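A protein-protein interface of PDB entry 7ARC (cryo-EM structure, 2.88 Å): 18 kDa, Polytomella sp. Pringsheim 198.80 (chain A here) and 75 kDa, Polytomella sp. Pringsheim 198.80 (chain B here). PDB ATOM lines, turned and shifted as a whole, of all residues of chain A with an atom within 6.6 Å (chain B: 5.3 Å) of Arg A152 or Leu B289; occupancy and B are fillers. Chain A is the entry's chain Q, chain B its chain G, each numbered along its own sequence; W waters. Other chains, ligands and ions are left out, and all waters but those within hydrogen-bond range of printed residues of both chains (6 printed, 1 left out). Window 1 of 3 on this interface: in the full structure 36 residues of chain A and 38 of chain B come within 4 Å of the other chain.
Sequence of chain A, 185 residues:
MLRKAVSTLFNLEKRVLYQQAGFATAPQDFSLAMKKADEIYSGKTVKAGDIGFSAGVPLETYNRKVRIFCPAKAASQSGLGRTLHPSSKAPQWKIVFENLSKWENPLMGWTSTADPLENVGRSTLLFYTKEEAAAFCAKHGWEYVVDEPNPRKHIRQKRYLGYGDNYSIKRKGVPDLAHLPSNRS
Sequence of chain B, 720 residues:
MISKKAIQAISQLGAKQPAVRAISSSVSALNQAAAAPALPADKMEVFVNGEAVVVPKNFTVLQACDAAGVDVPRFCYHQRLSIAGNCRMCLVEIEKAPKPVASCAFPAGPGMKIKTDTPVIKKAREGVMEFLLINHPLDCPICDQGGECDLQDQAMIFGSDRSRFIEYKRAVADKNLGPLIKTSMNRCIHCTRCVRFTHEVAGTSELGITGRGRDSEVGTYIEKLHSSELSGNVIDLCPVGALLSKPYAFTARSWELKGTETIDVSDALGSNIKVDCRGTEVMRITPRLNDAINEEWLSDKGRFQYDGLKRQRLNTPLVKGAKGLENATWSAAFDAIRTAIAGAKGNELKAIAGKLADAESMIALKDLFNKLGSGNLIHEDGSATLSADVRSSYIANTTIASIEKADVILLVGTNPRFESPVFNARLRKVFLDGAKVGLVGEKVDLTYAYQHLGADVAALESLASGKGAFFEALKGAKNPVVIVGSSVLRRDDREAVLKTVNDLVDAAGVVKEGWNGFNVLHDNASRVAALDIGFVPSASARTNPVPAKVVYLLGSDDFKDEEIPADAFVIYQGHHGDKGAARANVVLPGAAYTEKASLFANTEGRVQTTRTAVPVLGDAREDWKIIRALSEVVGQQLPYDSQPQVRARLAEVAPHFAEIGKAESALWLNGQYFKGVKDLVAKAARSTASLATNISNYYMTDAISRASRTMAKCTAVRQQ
Arg B74 touches Leu A80.
Asn A150 touches Asn B290.
CD2 of Leu B289 touches O of Pro A151, at 3.6 Å.
CD1 of Leu B289 touches CG of Arg A152, at 3.7 Å.
His A154 touches Asp B66 (NE2 to OD2, 3.9 Å).
Water W4 lies within hydrogen-bond range of OD2 of Asp B291 (2.4 Å), O of Lys A153 (2.8 Å) and NH2 of Arg B80 (3.0 Å).
Water W1 bridges OD2 of Asp B291 (2.5 Å) and O of Pro A151 (3.5 Å).
Water W6 bridges the side-chain amide oxygen (OE1) of Gln B79 (2.5 Å) and the guanidinium group (NE) of Arg A152 (2.9 Å).
Water W3 bridges O of Pro A151 (2.6 Å) and N of Asp B291 (3.1 Å).
Water W2 bridges O of Lys A73 (2.6 Å) and N of Leu B289 (3.1 Å).
Water W5 bridges the guanidinium group (NH1) of Arg B74 (3.2 Å) and the side-chain hydroxyl (OG) of Ser A78 (3.4 Å).
O of Asp B66 lies close to NE2 of His A85 (3.4 Å).
The guanidinium group (NH2) of Arg B74 is in hydrogen-bond range of the backbone carbonyl oxygen (O) of Ser A78, at 3.2 Å.
O of Lys A153 lies within hydrogen-bond range of NE2 of Gln B79.
OE1 of Gln B79 sits at hydrogen-bond distance from ND1 of His A154 (3.4 Å).
The guanidinium group (NH1) of Arg B288 lies within hydrogen-bond range of the side-chain amide oxygen (OD1) of Asn A150 (3.4 Å).
The side-chain amide oxygen (OD1) of Asn A150 sits close to the backbone carbonyl oxygen (O) of Leu B289 (3.1 Å).
Printed residues of chain B within 4 Å of Leu A80: Arg B74.
Printed residues of chain B within 4 Å of Arg A152: Leu B289 (3.7 Å).
Of the printed residues of chain A, Asp B66 touches His A85 and His A154.
Printed residues of chain A within 4 Å of Gln B79: Lys A153 (2.9 Å) and His A154 (3.4 Å).
Of the printed residues of chain A, Leu B289 touches Asn A150 (3.1 Å), Pro A151 (3.6 Å) and Arg A152 (3.7 Å).
Glu B295 touches none of the printed residues of chain A.
The nearest residue of chain A that does not touch Leu B289 is Ala A72 (5.2 Å).
Hydrophobic or aromatic side chains of chain A that line the printed part of chain B: Leu A80, His A85 and His A154.
Of the 12 printed residues of chain B, 6 touch a printed residue of chain A.
Hydrophobic or aromatic side chains of chain B that line the printed part of chain A: Leu B289.
Among the printed residues, 11 pairs touch across the chains.
Among the printed residues, no Asp or Glu carboxylate lies within 4 Å of a Lys or Arg side-chain nitrogen of the other chain.
The backbone carbonyl oxygen (O) of Arg B288 sits at hydrogen-bond distance from the side-chain amide nitrogen (ND2) of Asn B294, at 3.2 Å.
The backbone NH (N) of Asn B290 sits at hydrogen-bond distance from the backbone carbonyl oxygen (O) of Glu B295.
OG1 of Thr A83 sits at hydrogen-bond distance from O of Leu A80 (2.6 Å).
A ring nitrogen (ND1) of His A154 lies within hydrogen-bond range of the guanidinium group of Arg A152, 3.5 Å away.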
ATOM      1  N   ALA A  72       0.120  -5.179  30.588  1.00  0.00           N
ATOM      2  CA  ALA A  72       0.959  -6.355  30.443  1.00  0.00           C
ATOM      3  C   ALA A  72       0.910  -7.205  31.711  1.00  0.00           C
ATOM      4  O   ALA A  72       0.432  -6.778  32.765  1.00  0.00           O
ATOM      5  CB  ALA A  72       2.397  -5.954  30.122  1.00  0.00           C
ATOM      6  N   LYS A  73       1.412  -8.431  31.598  1.00  0.00           N
ATOM      7  CA  LYS A  73       1.414  -9.343  32.732  1.00  0.00           C
ATOM      8  C   LYS A  73       2.399  -8.869  33.792  1.00  0.00           C
ATOM      9  O   LYS A  73       3.500  -8.409  33.481  1.00  0.00           O
ATOM     10  CB  LYS A  73       1.784 -10.756  32.285  1.00  0.00           C
ATOM     11  CG  LYS A  73       1.762 -11.776  33.411  1.00  0.00           C
ATOM     12  CD  LYS A  73       2.005 -13.187  32.913  1.00  0.00           C
ATOM     13  CE  LYS A  73       3.455 -13.397  32.523  1.00  0.00           C
ATOM     14  NZ  LYS A  73       3.717 -14.814  32.147  1.00  0.00           N
ATOM     15  N   SER A  78       2.581 -15.806  37.157  1.00  0.00           N
ATOM     16  CA  SER A  78       2.590 -16.499  35.876  1.00  0.00           C
ATOM     17  C   SER A  78       1.194 -16.748  35.320  1.00  0.00           C
ATOM     18  O   SER A  78       1.060 -17.426  34.297  1.00  0.00           O
ATOM     19  CB  SER A  78       3.344 -17.824  36.000  1.00  0.00           C
ATOM     20  OG  SER A  78       4.708 -17.604  36.310  1.00  0.00           O
ATOM     21  N   LEU A  80      -2.203 -16.011  33.264  1.00  0.00           N
ATOM     22  CA  LEU A  80      -2.468 -15.350  31.993  1.00  0.00           C
ATOM     23  C   LEU A  80      -3.827 -14.667  31.943  1.00  0.00           C
ATOM     24  O   LEU A  80      -4.244 -14.228  30.867  1.00  0.00           O
ATOM     25  CB  LEU A  80      -2.358 -16.351  30.839  1.00  0.00           C
ATOM     26  CG  LEU A  80      -0.987 -16.687  30.246  1.00  0.00           C
ATOM     27  CD1 LEU A  80      -0.368 -15.456  29.606  1.00  0.00           C
ATOM     28  CD2 LEU A  80      -0.045 -17.295  31.270  1.00  0.00           C
ATOM     29  N   THR A  83      -3.719 -10.909  30.911  1.00  0.00           N
ATOM     30  CA  THR A  83      -3.230 -10.692  29.558  1.00  0.00           C
ATOM     31  C   THR A  83      -4.336 -10.921  28.532  1.00  0.00           C
ATOM     32  O   THR A  83      -5.345 -11.577  28.801  1.00  0.00           O
ATOM     33  CB  THR A  83      -2.063 -11.626  29.252  1.00  0.00           C
ATOM     34  OG1 THR A  83      -2.506 -12.984  29.342  1.00  0.00           O
ATOM     35  CG2 THR A  83      -0.951 -11.408  30.243  1.00  0.00           C
ATOM     36  N   LEU A  84      -4.112 -10.403  27.323  1.00  0.00           N
ATOM     37  CA  LEU A  84      -4.916 -10.805  26.175  1.00  0.00           C
ATOM     38  C   LEU A  84      -4.554 -12.220  25.757  1.00  0.00           C
ATOM     39  O   LEU A  84      -3.640 -12.429  24.954  1.00  0.00           O
ATOM     40  CB  LEU A  84      -4.731  -9.850  24.995  1.00  0.00           C
ATOM     41  CG  LEU A  84      -5.233  -8.416  25.145  1.00  0.00           C
ATOM     42  CD1 LEU A  84      -4.838  -7.593  23.938  1.00  0.00           C
ATOM     43  CD2 LEU A  84      -6.739  -8.405  25.329  1.00  0.00           C
ATOM     44  N   HIS A  85      -5.276 -13.190  26.298  1.00  0.00           N
ATOM     45  CA  HIS A  85      -5.085 -14.597  26.009  1.00  0.00           C
ATOM     46  C   HIS A  85      -6.445 -15.231  25.764  1.00  0.00           C
ATOM     47  O   HIS A  85      -7.454 -14.763  26.300  1.00  0.00           O
ATOM     48  CB  HIS A  85      -4.378 -15.292  27.182  1.00  0.00           C
ATOM     49  CG  HIS A  85      -3.785 -16.622  26.840  1.00  0.00           C
ATOM     50  ND1 HIS A  85      -4.343 -17.814  27.250  1.00  0.00           N
ATOM     51  CD2 HIS A  85      -2.679 -16.949  26.132  1.00  0.00           C
ATOM     52  CE1 HIS A  85      -3.608 -18.817  26.806  1.00  0.00           C
ATOM     53  NE2 HIS A  85      -2.593 -18.320  26.124  1.00  0.00           N
ATOM     54  N   PRO A 149      -0.460  -4.116  22.840  1.00  0.00           N
ATOM     55  CA  PRO A 149       0.430  -4.860  23.732  1.00  0.00           C
ATOM     56  C   PRO A 149       1.532  -5.544  22.940  1.00  0.00           C
ATOM     57  O   PRO A 149       1.352  -5.914  21.778  1.00  0.00           O
ATOM     58  CB  PRO A 149      -0.502  -5.879  24.396  1.00  0.00           C
ATOM     59  CG  PRO A 149      -1.648  -5.998  23.454  1.00  0.00           C
ATOM     60  CD  PRO A 149      -1.837  -4.626  22.899  1.00  0.00           C
ATOM     61  N   ASN A 150       2.683  -5.705  23.575  1.00  0.00           N
ATOM     62  CA  ASN A 150       3.765  -6.445  22.948  1.00  0.00           C
ATOM     63  C   ASN A 150       3.331  -7.895  22.759  1.00  0.00           C
ATOM     64  O   ASN A 150       2.875  -8.528  23.720  1.00  0.00           O
ATOM     65  CB  ASN A 150       5.034  -6.379  23.794  1.00  0.00           C
ATOM     66  CG  ASN A 150       5.497  -4.962  24.034  1.00  0.00           C
ATOM     67  OD1 ASN A 150       5.833  -4.588  25.157  1.00  0.00           O
ATOM     68  ND2 ASN A 150       5.514  -4.160  22.978  1.00  0.00           N
ATOM     69  N   PRO A 151       3.436  -8.447  21.550  1.00  0.00           N
ATOM     70  CA  PRO A 151       2.911  -9.795  21.311  1.00  0.00           C
ATOM     71  C   PRO A 151       3.610 -10.825  22.185  1.00  0.00           C
ATOM     72  O   PRO A 151       4.828 -10.791  22.368  1.00  0.00           O
ATOM     73  CB  PRO A 151       3.199 -10.025  19.824  1.00  0.00           C
ATOM     74  CG  PRO A 151       4.342  -9.113  19.528  1.00  0.00           C
ATOM     75  CD  PRO A 151       4.073  -7.889  20.346  1.00  0.00           C
ATOM     76  N   ARG A 152       2.820 -11.749  22.720  1.00  0.00           N
ATOM     77  CA  ARG A 152       3.321 -12.841  23.541  1.00  0.00           C
ATOM     78  C   ARG A 152       3.163 -14.150  22.782  1.00  0.00           C
ATOM     79  O   ARG A 152       2.039 -14.588  22.516  1.00  0.00           O
ATOM     80  CB  ARG A 152       2.568 -12.857  24.873  1.00  0.00           C
ATOM     81  CG  ARG A 152       3.020 -13.841  25.939  1.00  0.00           C
ATOM     82  CD  ARG A 152       2.247 -15.147  25.849  1.00  0.00           C
ATOM     83  NE  ARG A 152       2.553 -16.043  26.959  1.00  0.00           N
ATOM     84  CZ  ARG A 152       2.145 -17.301  27.044  1.00  0.00           C
ATOM     85  NH1 ARG A 152       1.344 -17.830  26.135  1.00  0.00           N
ATOM     86  NH2 ARG A 152       2.525 -18.038  28.084  1.00  0.00           N
ATOM     87  N   LYS A 153       4.290 -14.770  22.440  1.00  0.00           N
ATOM     88  CA  LYS A 153       4.320 -16.039  21.729  1.00  0.00           C
ATOM     89  C   LYS A 153       4.980 -17.078  22.619  1.00  0.00           C
ATOM     90  O   LYS A 153       6.103 -16.870  23.089  1.00  0.00           O
ATOM     91  CB  LYS A 153       5.075 -15.914  20.405  1.00  0.00           C
ATOM     92  CG  LYS A 153       4.706 -14.683  19.598  1.00  0.00           C
ATOM     93  CD  LYS A 153       3.255 -14.734  19.150  1.00  0.00           C
ATOM     94  CE  LYS A 153       2.890 -13.507  18.332  1.00  0.00           C
ATOM     95  NZ  LYS A 153       3.893 -13.227  17.269  1.00  0.00           N
ATOM     96  N   HIS A 154       4.288 -18.189  22.850  1.00  0.00           N
ATOM     97  CA  HIS A 154       4.768 -19.203  23.785  1.00  0.00           C
ATOM     98  C   HIS A 154       5.606 -20.230  23.021  1.00  0.00           C
ATOM     99  O   HIS A 154       5.215 -21.377  22.798  1.00  0.00           O
ATOM    100  CB  HIS A 154       3.595 -19.830  24.526  1.00  0.00           C
ATOM    101  CG  HIS A 154       3.997 -20.844  25.549  1.00  0.00           C
ATOM    102  ND1 HIS A 154       4.567 -20.496  26.754  1.00  0.00           N
ATOM    103  CD2 HIS A 154       3.875 -22.190  25.565  1.00  0.00           C
ATOM    104  CE1 HIS A 154       4.802 -21.589  27.458  1.00  0.00           C
ATOM    105  NE2 HIS A 154       4.390 -22.630  26.759  1.00  0.00           N
ATOM    106  N   ASP B  66      -2.402 -24.170  26.305  1.00  0.00           N
ATOM    107  CA  ASP B  66      -2.412 -22.712  26.214  1.00  0.00           C
ATOM    108  C   ASP B  66      -2.971 -22.247  24.877  1.00  0.00           C
ATOM    109  O   ASP B  66      -3.722 -21.268  24.817  1.00  0.00           O
ATOM    110  CB  ASP B  66      -1.006 -22.147  26.421  1.00  0.00           C
ATOM    111  CG  ASP B  66      -0.508 -22.316  27.840  1.00  0.00           C
ATOM    112  OD1 ASP B  66      -1.342 -22.340  28.769  1.00  0.00           O
ATOM    113  OD2 ASP B  66       0.723 -22.408  28.029  1.00  0.00           O
ATOM    114  N   ARG B  74       0.505 -24.184  37.109  1.00  0.00           N
ATOM    115  CA  ARG B  74       1.934 -24.428  36.993  1.00  0.00           C
ATOM    116  C   ARG B  74       2.649 -23.794  38.175  1.00  0.00           C
ATOM    117  O   ARG B  74       2.208 -22.776  38.711  1.00  0.00           O
ATOM    118  CB  ARG B  74       2.511 -23.859  35.692  1.00  0.00           C
ATOM    119  CG  ARG B  74       1.762 -24.256  34.445  1.00  0.00           C
ATOM    120  CD  ARG B  74       1.956 -23.224  33.358  1.00  0.00           C
ATOM    121  NE  ARG B  74       0.920 -22.201  33.401  1.00  0.00           N
ATOM    122  CZ  ARG B  74       1.014 -21.020  32.810  1.00  0.00           C
ATOM    123  NH1 ARG B  74       2.090 -20.675  32.124  1.00  0.00           N
ATOM    124  NH2 ARG B  74       0.004 -20.161  32.914  1.00  0.00           N
ATOM    125  N   GLN B  79       8.600 -20.519  30.521  1.00  0.00           N
ATOM    126  CA  GLN B  79       8.731 -20.554  29.072  1.00  0.00           C
ATOM    127  C   GLN B  79      10.187 -20.453  28.653  1.00  0.00           C
ATOM    128  O   GLN B  79      10.618 -21.105  27.696  1.00  0.00           O
ATOM    129  CB  GLN B  79       7.920 -19.422  28.450  1.00  0.00           C
ATOM    130  CG  GLN B  79       7.977 -19.385  26.942  1.00  0.00           C
ATOM    131  CD  GLN B  79       7.348 -18.135  26.371  1.00  0.00           C
ATOM    132  OE1 GLN B  79       6.377 -17.612  26.915  1.00  0.00           O
ATOM    133  NE2 GLN B  79       7.900 -17.649  25.267  1.00  0.00           N
ATOM    134  N   ARG B  80      10.957 -19.632  29.358  1.00  0.00           N
ATOM    135  CA  ARG B  80      12.307 -19.292  28.953  1.00  0.00           C
ATOM    136  C   ARG B  80      13.357 -20.071  29.734  1.00  0.00           C
ATOM    137  O   ARG B  80      14.548 -19.770  29.629  1.00  0.00           O
ATOM    138  CB  ARG B  80      12.492 -17.789  29.124  1.00  0.00           C
ATOM    139  CG  ARG B  80      11.568 -17.071  28.167  1.00  0.00           C
ATOM    140  CD  ARG B  80      11.643 -15.573  28.176  1.00  0.00           C
ATOM    141  NE  ARG B  80      10.606 -15.054  27.293  1.00  0.00           N
ATOM    142  CZ  ARG B  80      10.743 -14.850  25.992  1.00  0.00           C
ATOM    143  NH1 ARG B  80      11.891 -15.060  25.375  1.00  0.00           N
ATOM    144  NH2 ARG B  80       9.699 -14.420  25.291  1.00  0.00           N
ATOM    145  N   PRO B 287      10.232  -5.640  35.159  1.00  0.00           N
ATOM    146  CA  PRO B 287      10.253  -5.688  33.694  1.00  0.00           C
ATOM    147  C   PRO B 287       8.883  -5.988  33.105  1.00  0.00           C
ATOM    148  O   PRO B 287       7.933  -6.370  33.789  1.00  0.00           O
ATOM    149  CB  PRO B 287      11.243  -6.816  33.405  1.00  0.00           C
ATOM    150  CG  PRO B 287      11.082  -7.719  34.564  1.00  0.00           C
ATOM    151  CD  PRO B 287      10.931  -6.800  35.739  1.00  0.00           C
ATOM    152  N   ARG B 288       8.802  -5.804  31.791  1.00  0.00           N
ATOM    153  CA  ARG B 288       7.652  -6.190  30.991  1.00  0.00           C
ATOM    154  C   ARG B 288       8.131  -7.097  29.870  1.00  0.00           C
ATOM    155  O   ARG B 288       9.318  -7.136  29.541  1.00  0.00           O
ATOM    156  CB  ARG B 288       6.897  -5.000  30.385  1.00  0.00           C
ATOM    157  CG  ARG B 288       6.177  -4.134  31.381  1.00  0.00           C
ATOM    158  CD  ARG B 288       5.387  -3.034  30.694  1.00  0.00           C
ATOM    159  NE  ARG B 288       6.216  -2.014  30.063  1.00  0.00           N
ATOM    160  CZ  ARG B 288       6.288  -1.813  28.755  1.00  0.00           C
ATOM    161  NH1 ARG B 288       5.572  -2.529  27.906  1.00  0.00           N
ATOM    162  NH2 ARG B 288       7.076  -0.850  28.288  1.00  0.00           N
ATOM    163  N   LEU B 289       7.192  -7.825  29.280  1.00  0.00           N
ATOM    164  CA  LEU B 289       7.515  -8.749  28.205  1.00  0.00           C
ATOM    165  C   LEU B 289       7.659  -7.973  26.904  1.00  0.00           C
ATOM    166  O   LEU B 289       6.725  -7.292  26.470  1.00  0.00           O
ATOM    167  CB  LEU B 289       6.439  -9.827  28.092  1.00  0.00           C
ATOM    168  CG  LEU B 289       6.644 -11.013  27.147  1.00  0.00           C
ATOM    169  CD1 LEU B 289       5.861 -12.203  27.657  1.00  0.00           C
ATOM    170  CD2 LEU B 289       6.194 -10.681  25.738  1.00  0.00           C
ATOM    171  N   ASN B 290       8.841  -8.066  26.296  1.00  0.00           N
ATOM    172  CA  ASN B 290       9.056  -7.591  24.932  1.00  0.00           C
ATOM    173  C   ASN B 290      10.120  -8.480  24.299  1.00  0.00           C
ATOM    174  O   ASN B 290      11.315  -8.238  24.476  1.00  0.00           O
ATOM    175  CB  ASN B 290       9.481  -6.131  24.920  1.00  0.00           C
ATOM    176  CG  ASN B 290       9.175  -5.446  23.608  1.00  0.00           C
ATOM    177  OD1 ASN B 290       8.909  -6.099  22.601  1.00  0.00           O
ATOM    178  ND2 ASN B 290       9.222  -4.123  23.609  1.00  0.00           N
ATOM    179  N   ASP B 291       9.675  -9.494  23.554  1.00  0.00           N
ATOM    180  CA  ASP B 291      10.606 -10.444  22.954  1.00  0.00           C
ATOM    181  C   ASP B 291      11.614  -9.744  22.055  1.00  0.00           C
ATOM    182  O   ASP B 291      12.719 -10.253  21.844  1.00  0.00           O
ATOM    183  CB  ASP B 291       9.836 -11.499  22.166  1.00  0.00           C
ATOM    184  CG  ASP B 291       9.043 -12.418  23.060  1.00  0.00           C
ATOM    185  OD1 ASP B 291       9.259 -12.375  24.288  1.00  0.00           O
ATOM    186  OD2 ASP B 291       8.202 -13.181  22.540  1.00  0.00           O
ATOM    187  N   ASN B 294      14.016  -6.941  25.593  1.00  0.00           N
ATOM    188  CA  ASN B 294      14.231  -7.684  26.830  1.00  0.00           C
ATOM    189  C   ASN B 294      13.146  -8.744  26.925  1.00  0.00           C
ATOM    190  O   ASN B 294      11.966  -8.407  27.064  1.00  0.00           O
ATOM    191  CB  ASN B 294      14.225  -6.763  28.050  1.00  0.00           C
ATOM    192  CG  ASN B 294      12.928  -6.003  28.205  1.00  0.00           C
ATOM    193  OD1 ASN B 294      12.438  -5.387  27.262  1.00  0.00           O
ATOM    194  ND2 ASN B 294      12.357  -6.053  29.399  1.00  0.00           N
ATOM    195  N   GLU B 295      13.531 -10.013  26.802  1.00  0.00           N
ATOM    196  CA  GLU B 295      12.550 -11.090  26.817  1.00  0.00           C
ATOM    197  C   GLU B 295      11.593 -10.884  27.982  1.00  0.00           C
ATOM    198  O   GLU B 295      10.414 -10.579  27.782  1.00  0.00           O
ATOM    199  CB  GLU B 295      13.255 -12.437  26.940  1.00  0.00           C
ATOM    200  CG  GLU B 295      14.377 -12.621  25.949  1.00  0.00           C
ATOM    201  CD  GLU B 295      14.599 -14.068  25.595  1.00  0.00           C
ATOM    202  OE1 GLU B 295      14.529 -14.925  26.501  1.00  0.00           O
ATOM    203  OE2 GLU B 295      14.812 -14.358  24.401  1.00  0.00           O
ATOM    204  N   GLU B 296      12.097 -11.047  29.202  1.00  0.00           N
ATOM    205  CA  GLU B 296      11.391 -10.537  30.372  1.00  0.00           C
ATOM    206  C   GLU B 296      12.375 -10.177  31.481  1.00  0.00           C
ATOM    207  O   GLU B 296      11.963 -10.071  32.641  1.00  0.00           O
ATOM    208  CB  GLU B 296      10.328 -11.500  30.881  1.00  0.00           C
ATOM    209  CG  GLU B 296      10.811 -12.808  31.418  1.00  0.00           C
ATOM    210  CD  GLU B 296       9.646 -13.678  31.814  1.00  0.00           C
ATOM    211  OE1 GLU B 296       8.490 -13.241  31.636  1.00  0.00           O
ATOM    212  OE2 GLU B 296       9.875 -14.775  32.342  1.00  0.00           O
HETATM  213  O   HOH W   1       7.080 -12.613  20.420  1.00  0.00           O
HETATM  214  O   HOH W   2       4.841  -8.497  31.216  1.00  0.00           O
HETATM  215  O   HOH W   3       6.956  -9.294  22.174  1.00  0.00           O
HETATM  216  O   HOH W   4       6.922 -14.410  24.201  1.00  0.00           O
HETATM  217  O   HOH W   5       4.700 -19.840  33.704  1.00  0.00           O
HETATM  218  O   HOH W   6       5.289 -15.626  27.959  1.00  0.00           O
